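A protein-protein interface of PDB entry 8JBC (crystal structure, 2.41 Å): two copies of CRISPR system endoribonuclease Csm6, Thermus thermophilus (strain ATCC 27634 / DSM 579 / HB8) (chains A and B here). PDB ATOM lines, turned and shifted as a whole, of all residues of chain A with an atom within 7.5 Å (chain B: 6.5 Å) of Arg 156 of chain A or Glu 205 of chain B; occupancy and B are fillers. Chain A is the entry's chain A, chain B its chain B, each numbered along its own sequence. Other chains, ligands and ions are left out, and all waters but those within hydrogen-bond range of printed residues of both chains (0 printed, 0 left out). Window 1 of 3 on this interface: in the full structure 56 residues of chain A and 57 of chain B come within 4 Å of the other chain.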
ATOM      1  N   ALA A 150      17.285  23.515 -38.228  1.00  0.00           N
ATOM      2  CA  ALA A 150      17.640  24.374 -37.109  1.00  0.00           C
ATOM      3  C   ALA A 150      16.700  25.565 -37.022  1.00  0.00           C
ATOM      4  O   ALA A 150      16.230  25.918 -35.934  1.00  0.00           O
ATOM      5  CB  ALA A 150      19.084  24.853 -37.262  1.00  0.00           C
ATOM      6  N   GLY A 151      16.414  26.196 -38.170  1.00  0.00           N
ATOM      7  CA  GLY A 151      15.576  27.383 -38.160  1.00  0.00           C
ATOM      8  C   GLY A 151      14.220  27.097 -37.552  1.00  0.00           C
ATOM      9  O   GLY A 151      13.749  27.826 -36.677  1.00  0.00           O
ATOM     10  N   PHE A 152      13.605  25.986 -37.960  1.00  0.00           N
ATOM     11  CA  PHE A 152      12.232  25.730 -37.532  1.00  0.00           C
ATOM     12  C   PHE A 152      12.189  25.287 -36.091  1.00  0.00           C
ATOM     13  O   PHE A 152      11.303  25.706 -35.342  1.00  0.00           O
ATOM     14  CB  PHE A 152      11.561  24.700 -38.433  1.00  0.00           C
ATOM     15  CG  PHE A 152      11.302  25.222 -39.796  1.00  0.00           C
ATOM     16  CD1 PHE A 152      10.887  26.559 -39.970  1.00  0.00           C
ATOM     17  CD2 PHE A 152      11.536  24.440 -40.913  1.00  0.00           C
ATOM     18  CE1 PHE A 152      10.644  27.078 -41.240  1.00  0.00           C
ATOM     19  CE2 PHE A 152      11.303  24.967 -42.185  1.00  0.00           C
ATOM     20  CZ  PHE A 152      10.860  26.283 -42.349  1.00  0.00           C
ATOM     21  N   PHE A 153      13.134  24.444 -35.693  1.00  0.00           N
ATOM     22  CA  PHE A 153      13.241  24.067 -34.293  1.00  0.00           C
ATOM     23  C   PHE A 153      13.443  25.299 -33.421  1.00  0.00           C
ATOM     24  O   PHE A 153      12.761  25.480 -32.416  1.00  0.00           O
ATOM     25  CB  PHE A 153      14.394  23.089 -34.112  1.00  0.00           C
ATOM     26  CG  PHE A 153      14.686  22.759 -32.692  1.00  0.00           C
ATOM     27  CD1 PHE A 153      13.999  21.729 -32.057  1.00  0.00           C
ATOM     28  CD2 PHE A 153      15.670  23.447 -31.988  1.00  0.00           C
ATOM     29  CE1 PHE A 153      14.262  21.384 -30.735  1.00  0.00           C
ATOM     30  CE2 PHE A 153      15.953  23.113 -30.651  1.00  0.00           C
ATOM     31  CZ  PHE A 153      15.242  22.075 -30.035  1.00  0.00           C
ATOM     32  N   PHE A 154      14.360  26.178 -33.811  1.00  0.00           N
ATOM     33  CA  PHE A 154      14.648  27.277 -32.925  1.00  0.00           C
ATOM     34  C   PHE A 154      13.531  28.317 -32.884  1.00  0.00           C
ATOM     35  O   PHE A 154      13.519  29.143 -31.960  1.00  0.00           O
ATOM     36  CB  PHE A 154      15.980  27.885 -33.321  1.00  0.00           C
ATOM     37  CG  PHE A 154      17.146  27.155 -32.742  1.00  0.00           C
ATOM     38  CD1 PHE A 154      17.311  27.084 -31.369  1.00  0.00           C
ATOM     39  CD2 PHE A 154      18.059  26.519 -33.547  1.00  0.00           C
ATOM     40  CE1 PHE A 154      18.367  26.407 -30.812  1.00  0.00           C
ATOM     41  CE2 PHE A 154      19.138  25.838 -32.984  1.00  0.00           C
ATOM     42  CZ  PHE A 154      19.288  25.780 -31.616  1.00  0.00           C
ATOM     43  N   GLN A 155      12.575  28.262 -33.826  1.00  0.00           N
ATOM     44  CA  GLN A 155      11.495  29.246 -33.862  1.00  0.00           C
ATOM     45  C   GLN A 155      10.651  29.194 -32.605  1.00  0.00           C
ATOM     46  O   GLN A 155      10.103  30.211 -32.181  1.00  0.00           O
ATOM     47  CB  GLN A 155      10.608  29.020 -35.081  1.00  0.00           C
ATOM     48  CG  GLN A 155      10.888  29.982 -36.210  1.00  0.00           C
ATOM     49  CD  GLN A 155       9.967  29.721 -37.377  1.00  0.00           C
ATOM     50  OE1 GLN A 155       9.191  28.747 -37.344  1.00  0.00           O
ATOM     51  NE2 GLN A 155      10.055  30.558 -38.432  1.00  0.00           N
ATOM     52  N   ARG A 156      10.523  28.012 -32.019  1.00  0.00           N
ATOM     53  CA  ARG A 156       9.862  27.865 -30.733  1.00  0.00           C
ATOM     54  C   ARG A 156      10.407  28.849 -29.704  1.00  0.00           C
ATOM     55  O   ARG A 156       9.657  29.405 -28.901  1.00  0.00           O
ATOM     56  CB  ARG A 156      10.077  26.438 -30.255  1.00  0.00           C
ATOM     57  CG  ARG A 156       9.661  26.174 -28.870  1.00  0.00           C
ATOM     58  CD  ARG A 156       9.682  24.694 -28.653  1.00  0.00           C
ATOM     59  NE  ARG A 156       9.133  24.345 -27.356  1.00  0.00           N
ATOM     60  CZ  ARG A 156       8.659  23.144 -27.050  1.00  0.00           C
ATOM     61  NH1 ARG A 156       8.641  22.165 -27.941  1.00  0.00           N
ATOM     62  NH2 ARG A 156       8.199  22.923 -25.824  1.00  0.00           N
ATOM     63  N   PHE A 157      11.711  29.061 -29.701  1.00  0.00           N
ATOM     64  CA  PHE A 157      12.322  29.929 -28.725  1.00  0.00           C
ATOM     65  C   PHE A 157      12.668  31.283 -29.278  1.00  0.00           C
ATOM     66  O   PHE A 157      12.839  32.212 -28.491  1.00  0.00           O
ATOM     67  CB  PHE A 157      13.598  29.294 -28.172  1.00  0.00           C
ATOM     68  CG  PHE A 157      13.427  27.884 -27.789  1.00  0.00           C
ATOM     69  CD1 PHE A 157      12.696  27.546 -26.653  1.00  0.00           C
ATOM     70  CD2 PHE A 157      13.966  26.874 -28.570  1.00  0.00           C
ATOM     71  CE1 PHE A 157      12.532  26.225 -26.292  1.00  0.00           C
ATOM     72  CE2 PHE A 157      13.798  25.525 -28.207  1.00  0.00           C
ATOM     73  CZ  PHE A 157      13.076  25.209 -27.071  1.00  0.00           C
ATOM     74  N   TYR A 158      12.799  31.413 -30.598  1.00  0.00           N
ATOM     75  CA  TYR A 158      13.182  32.670 -31.247  1.00  0.00           C
ATOM     76  C   TYR A 158      12.190  32.942 -32.360  1.00  0.00           C
ATOM     77  O   TYR A 158      12.467  32.658 -33.535  1.00  0.00           O
ATOM     78  CB  TYR A 158      14.602  32.614 -31.795  1.00  0.00           C
ATOM     79  CG  TYR A 158      15.648  32.324 -30.739  1.00  0.00           C
ATOM     80  CD1 TYR A 158      15.921  31.014 -30.345  1.00  0.00           C
ATOM     81  CD2 TYR A 158      16.361  33.366 -30.124  1.00  0.00           C
ATOM     82  CE1 TYR A 158      16.876  30.741 -29.372  1.00  0.00           C
ATOM     83  CE2 TYR A 158      17.323  33.097 -29.160  1.00  0.00           C
ATOM     84  CZ  TYR A 158      17.570  31.783 -28.785  1.00  0.00           C
ATOM     85  OH  TYR A 158      18.518  31.507 -27.827  1.00  0.00           O
ATOM     86  N   PRO A 159      11.020  33.493 -32.021  1.00  0.00           N
ATOM     87  CA  PRO A 159       9.929  33.637 -33.013  1.00  0.00           C
ATOM     88  C   PRO A 159      10.252  34.539 -34.190  1.00  0.00           C
ATOM     89  O   PRO A 159       9.523  34.506 -35.186  1.00  0.00           O
ATOM     90  CB  PRO A 159       8.766  34.224 -32.201  1.00  0.00           C
ATOM     91  CG  PRO A 159       9.309  34.547 -30.816  1.00  0.00           C
ATOM     92  CD  PRO A 159      10.631  33.855 -30.643  1.00  0.00           C
ATOM     93  N   VAL A 161      12.881  34.355 -36.099  1.00  0.00           N
ATOM     94  CA  VAL A 161      13.657  33.638 -37.109  1.00  0.00           C
ATOM     95  C   VAL A 161      12.793  33.299 -38.314  1.00  0.00           C
ATOM     96  O   VAL A 161      11.637  32.858 -38.177  1.00  0.00           O
ATOM     97  CB  VAL A 161      14.244  32.348 -36.524  1.00  0.00           C
ATOM     98  CG1 VAL A 161      14.948  31.558 -37.625  1.00  0.00           C
ATOM     99  CG2 VAL A 161      15.157  32.684 -35.389  1.00  0.00           C
ATOM    100  N   ASN A 190       7.187  27.332 -42.187  1.00  0.00           N
ATOM    101  CA  ASN A 190       7.195  26.257 -41.204  1.00  0.00           C
ATOM    102  C   ASN A 190       6.064  25.278 -41.537  1.00  0.00           C
ATOM    103  O   ASN A 190       4.962  25.705 -41.885  1.00  0.00           O
ATOM    104  CB  ASN A 190       6.993  26.872 -39.812  1.00  0.00           C
ATOM    105  CG  ASN A 190       7.181  25.902 -38.702  1.00  0.00           C
ATOM    106  OD1 ASN A 190       6.580  24.826 -38.681  1.00  0.00           O
ATOM    107  ND2 ASN A 190       8.043  26.269 -37.745  1.00  0.00           N
ATOM    108  N   ARG B 156       7.378  14.378 -33.910  1.00  0.00           N
ATOM    109  CA  ARG B 156       6.674  14.540 -32.641  1.00  0.00           C
ATOM    110  C   ARG B 156       5.446  13.635 -32.536  1.00  0.00           C
ATOM    111  O   ARG B 156       5.124  13.140 -31.451  1.00  0.00           O
ATOM    112  CB  ARG B 156       6.268  15.991 -32.478  1.00  0.00           C
ATOM    113  CG  ARG B 156       5.423  16.275 -31.275  1.00  0.00           C
ATOM    114  CD  ARG B 156       5.131  17.761 -31.218  1.00  0.00           C
ATOM    115  NE  ARG B 156       4.222  18.074 -30.137  1.00  0.00           N
ATOM    116  CZ  ARG B 156       4.174  19.241 -29.514  1.00  0.00           C
ATOM    117  NH1 ARG B 156       4.947  20.252 -29.878  1.00  0.00           N
ATOM    118  NH2 ARG B 156       3.332  19.395 -28.495  1.00  0.00           N
ATOM    119  N   ALA B 200      18.424  23.019 -21.838  1.00  0.00           N
ATOM    120  CA  ALA B 200      18.379  24.268 -21.092  1.00  0.00           C
ATOM    121  C   ALA B 200      17.355  25.243 -21.679  1.00  0.00           C
ATOM    122  O   ALA B 200      16.769  26.048 -20.942  1.00  0.00           O
ATOM    123  CB  ALA B 200      19.769  24.891 -21.027  1.00  0.00           C
ATOM    124  N   LEU B 201      17.103  25.185 -22.982  1.00  0.00           N
ATOM    125  CA  LEU B 201      16.059  26.046 -23.545  1.00  0.00           C
ATOM    126  C   LEU B 201      14.674  25.517 -23.178  1.00  0.00           C
ATOM    127  O   LEU B 201      13.766  26.291 -22.852  1.00  0.00           O
ATOM    128  CB  LEU B 201      16.221  26.160 -25.075  1.00  0.00           C
ATOM    129  CG  LEU B 201      17.179  27.226 -25.644  1.00  0.00           C
ATOM    130  CD1 LEU B 201      18.454  27.366 -24.820  1.00  0.00           C
ATOM    131  CD2 LEU B 201      17.570  26.859 -27.049  1.00  0.00           C
ATOM    132  N   PHE B 202      14.498  24.196 -23.206  1.00  0.00           N
ATOM    133  CA  PHE B 202      13.217  23.638 -22.787  1.00  0.00           C
ATOM    134  C   PHE B 202      12.917  24.007 -21.348  1.00  0.00           C
ATOM    135  O   PHE B 202      11.788  24.399 -21.020  1.00  0.00           O
ATOM    136  CB  PHE B 202      13.212  22.117 -22.952  1.00  0.00           C
ATOM    137  CG  PHE B 202      13.168  21.682 -24.378  1.00  0.00           C
ATOM    138  CD1 PHE B 202      12.136  22.103 -25.200  1.00  0.00           C
ATOM    139  CD2 PHE B 202      14.192  20.904 -24.918  1.00  0.00           C
ATOM    140  CE1 PHE B 202      12.114  21.739 -26.544  1.00  0.00           C
ATOM    141  CE2 PHE B 202      14.174  20.533 -26.253  1.00  0.00           C
ATOM    142  CZ  PHE B 202      13.130  20.951 -27.065  1.00  0.00           C
ATOM    143  N   ALA B 203      13.926  23.892 -20.478  1.00  0.00           N
ATOM    144  CA  ALA B 203      13.726  24.161 -19.058  1.00  0.00           C
ATOM    145  C   ALA B 203      13.336  25.614 -18.832  1.00  0.00           C
ATOM    146  O   ALA B 203      12.353  25.891 -18.141  1.00  0.00           O
ATOM    147  CB  ALA B 203      14.989  23.789 -18.266  1.00  0.00           C
ATOM    148  N   LYS B 204      14.045  26.548 -19.476  1.00  0.00           N
ATOM    149  CA  LYS B 204      13.719  27.961 -19.342  1.00  0.00           C
ATOM    150  C   LYS B 204      12.310  28.271 -19.834  1.00  0.00           C
ATOM    151  O   LYS B 204      11.563  29.038 -19.211  1.00  0.00           O
ATOM    152  CB  LYS B 204      14.726  28.801 -20.105  1.00  0.00           C
ATOM    153  CG  LYS B 204      14.277  30.228 -20.249  1.00  0.00           C
ATOM    154  CD  LYS B 204      15.387  31.078 -20.833  1.00  0.00           C
ATOM    155  CE  LYS B 204      14.891  32.487 -21.050  1.00  0.00           C
ATOM    156  NZ  LYS B 204      15.802  33.177 -21.990  1.00  0.00           N
ATOM    157  N   GLU B 205      11.920  27.690 -20.950  1.00  0.00           N
ATOM    158  CA  GLU B 205      10.550  27.895 -21.380  1.00  0.00           C
ATOM    159  C   GLU B 205       9.570  27.372 -20.332  1.00  0.00           C
ATOM    160  O   GLU B 205       8.609  28.061 -19.976  1.00  0.00           O
ATOM    161  CB  GLU B 205      10.334  27.233 -22.736  1.00  0.00           C
ATOM    162  CG  GLU B 205       9.020  27.544 -23.354  1.00  0.00           C
ATOM    163  CD  GLU B 205       8.969  27.072 -24.789  1.00  0.00           C
ATOM    164  OE1 GLU B 205       8.670  25.882 -24.993  1.00  0.00           O
ATOM    165  OE2 GLU B 205       9.270  27.894 -25.703  1.00  0.00           O
ATOM    166  N   LEU B 206       9.791  26.148 -19.820  1.00  0.00           N
ATOM    167  CA  LEU B 206       8.837  25.600 -18.853  1.00  0.00           C
ATOM    168  C   LEU B 206       8.827  26.433 -17.576  1.00  0.00           C
ATOM    169  O   LEU B 206       7.768  26.685 -16.984  1.00  0.00           O
ATOM    170  CB  LEU B 206       9.165  24.147 -18.530  1.00  0.00           C
ATOM    171  CG  LEU B 206       8.864  23.107 -19.609  1.00  0.00           C
ATOM    172  CD1 LEU B 206       9.661  21.826 -19.359  1.00  0.00           C
ATOM    173  CD2 LEU B 206       7.382  22.806 -19.706  1.00  0.00           C
ATOM    174  N   TYR B 207      10.012  26.856 -17.140  1.00  0.00           N
ATOM    175  CA  TYR B 207      10.126  27.757 -16.010  1.00  0.00           C
ATOM    176  C   TYR B 207       9.225  28.972 -16.205  1.00  0.00           C
ATOM    177  O   TYR B 207       8.395  29.289 -15.347  1.00  0.00           O
ATOM    178  CB  TYR B 207      11.590  28.155 -15.861  1.00  0.00           C
ATOM    179  CG  TYR B 207      11.903  29.059 -14.713  1.00  0.00           C
ATOM    180  CD1 TYR B 207      11.820  30.431 -14.844  1.00  0.00           C
ATOM    181  CD2 TYR B 207      12.324  28.539 -13.499  1.00  0.00           C
ATOM    182  CE1 TYR B 207      12.132  31.265 -13.787  1.00  0.00           C
ATOM    183  CE2 TYR B 207      12.627  29.358 -12.443  1.00  0.00           C
ATOM    184  CZ  TYR B 207      12.538  30.718 -12.579  1.00  0.00           C
ATOM    185  OH  TYR B 207      12.866  31.530 -11.502  1.00  0.00           O
ATOM    186  N   GLY B 208       9.330  29.618 -17.363  1.00  0.00           N
ATOM    187  CA  GLY B 208       8.552  30.819 -17.614  1.00  0.00           C
ATOM    188  C   GLY B 208       7.055  30.588 -17.607  1.00  0.00           C
ATOM    189  O   GLY B 208       6.294  31.509 -17.330  1.00  0.00           O
ATOM    190  N   LYS B 209       6.611  29.363 -17.893  1.00  0.00           N
ATOM    191  CA  LYS B 209       5.195  28.992 -17.837  1.00  0.00           C
ATOM    192  C   LYS B 209       4.726  28.584 -16.435  1.00  0.00           C
ATOM    193  O   LYS B 209       3.555  28.216 -16.265  1.00  0.00           O
ATOM    194  CB  LYS B 209       4.914  27.824 -18.795  1.00  0.00           C
ATOM    195  CG  LYS B 209       4.981  28.126 -20.301  1.00  0.00           C
ATOM    196  CD  LYS B 209       4.286  26.987 -21.070  1.00  0.00           C
ATOM    197  CE  LYS B 209       4.894  26.749 -22.447  1.00  0.00           C
ATOM    198  NZ  LYS B 209       4.808  27.948 -23.333  1.00  0.00           N
ATOM    199  N   GLY B 210       5.600  28.589 -15.433  1.00  0.00           N
ATOM    200  CA  GLY B 210       5.214  28.046 -14.144  1.00  0.00           C
ATOM    201  C   GLY B 210       5.196  26.536 -14.064  1.00  0.00           C
ATOM    202  O   GLY B 210       4.695  25.987 -13.077  1.00  0.00           O
ATOM    203  N   GLU B 211       5.714  25.834 -15.070  1.00  0.00           N
ATOM    204  CA  GLU B 211       5.871  24.381 -14.983  1.00  0.00           C
ATOM    205  C   GLU B 211       7.175  24.056 -14.242  1.00  0.00           C
ATOM    206  O   GLU B 211       8.137  23.524 -14.794  1.00  0.00           O
ATOM    207  CB  GLU B 211       5.842  23.771 -16.380  1.00  0.00           C
ATOM    208  CG  GLU B 211       4.462  23.825 -17.052  1.00  0.00           C
ATOM    209  CD  GLU B 211       3.466  22.830 -16.409  1.00  0.00           C
ATOM    210  OE1 GLU B 211       3.742  21.609 -16.392  1.00  0.00           O
ATOM    211  OE2 GLU B 211       2.409  23.270 -15.893  1.00  0.00           O
ATOM    212  N   LEU B 466      15.945  33.921 -14.760  1.00  0.00           N
ATOM    213  CA  LEU B 466      17.052  32.975 -14.701  1.00  0.00           C
ATOM    214  C   LEU B 466      18.369  33.619 -15.118  1.00  0.00           C
ATOM    215  O   LEU B 466      19.442  33.130 -14.724  1.00  0.00           O
ATOM    216  CB  LEU B 466      16.751  31.777 -15.590  1.00  0.00           C
ATOM    217  CG  LEU B 466      15.488  30.970 -15.305  1.00  0.00           C
ATOM    218  CD1 LEU B 466      15.176  30.092 -16.515  1.00  0.00           C
ATOM    219  CD2 LEU B 466      15.650  30.129 -14.074  1.00  0.00           C
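Arg 156 of chain A touches just these residues of chain B: Phe 202 (3.8 Å) and Glu 205 (2.9 Å).
Glu 205 of chain B touches just these residues of chain A: Arg 156 and Phe 157.
Of the printed residues of chain A, Leu 201 of chain B touches Phe 154 (3.9 Å) and Phe 157 (3.7 Å).
Of the printed residues of chain A, Phe 202 of chain B touches Phe 153, Arg 156 and Phe 157.
Printed residues of chain B within 4 Å of Phe 157 of chain A: Leu 201, Phe 202 and Glu 205.
Asn 190 of chain A touches none of the printed residues of chain B.
Tyr 207 of chain B touches none of the printed residues of chain A.
The nearest printed residue of chain A that does not touch Phe 202 of chain B is Phe 154 of chain A (8.4 Å).
Position printed for both chains: 156.
Of the 7 pairs that touch across the chains among the printed residues, none has its exchanged pair printed and touching as well.
Among the printed residues, pairs that only touch across the chains: Phe 157 of chain A with Glu 205 of chain B (3.6 Å), Phe 157 of chain A with Phe 202 of chain B (3.6 Å), Phe 157 of chain A with Leu 201 of chain B (3.7 Å), Arg 156 of chain A with Phe 202 of chain B (3.8 Å), Phe 153 of chain A with Phe 202 of chain B (3.8 Å) and Phe 154 of chain A with Leu 201 of chain B (3.9 Å).
The guanidinium group (NE) of Arg 156 of chain A lies within salt-bridge range of the side-chain carboxylate (OE1) of Glu 205 of chain B (2.9 Å).
Of the 12 printed residues of chain A, 4 touch a printed residue of chain B.
Hydrophobic or aromatic side chains of chain A within 4 Å of the printed part of chain B: Phe 153, Phe 154 and Phe 157.
Printed residues of chain B that touch a printed residue of chain A: Leu 201, Phe 202 and Glu 205.
Hydrophobic or aromatic side chains of chain B that line the printed part of chain A: Leu 201 and Phe 202.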
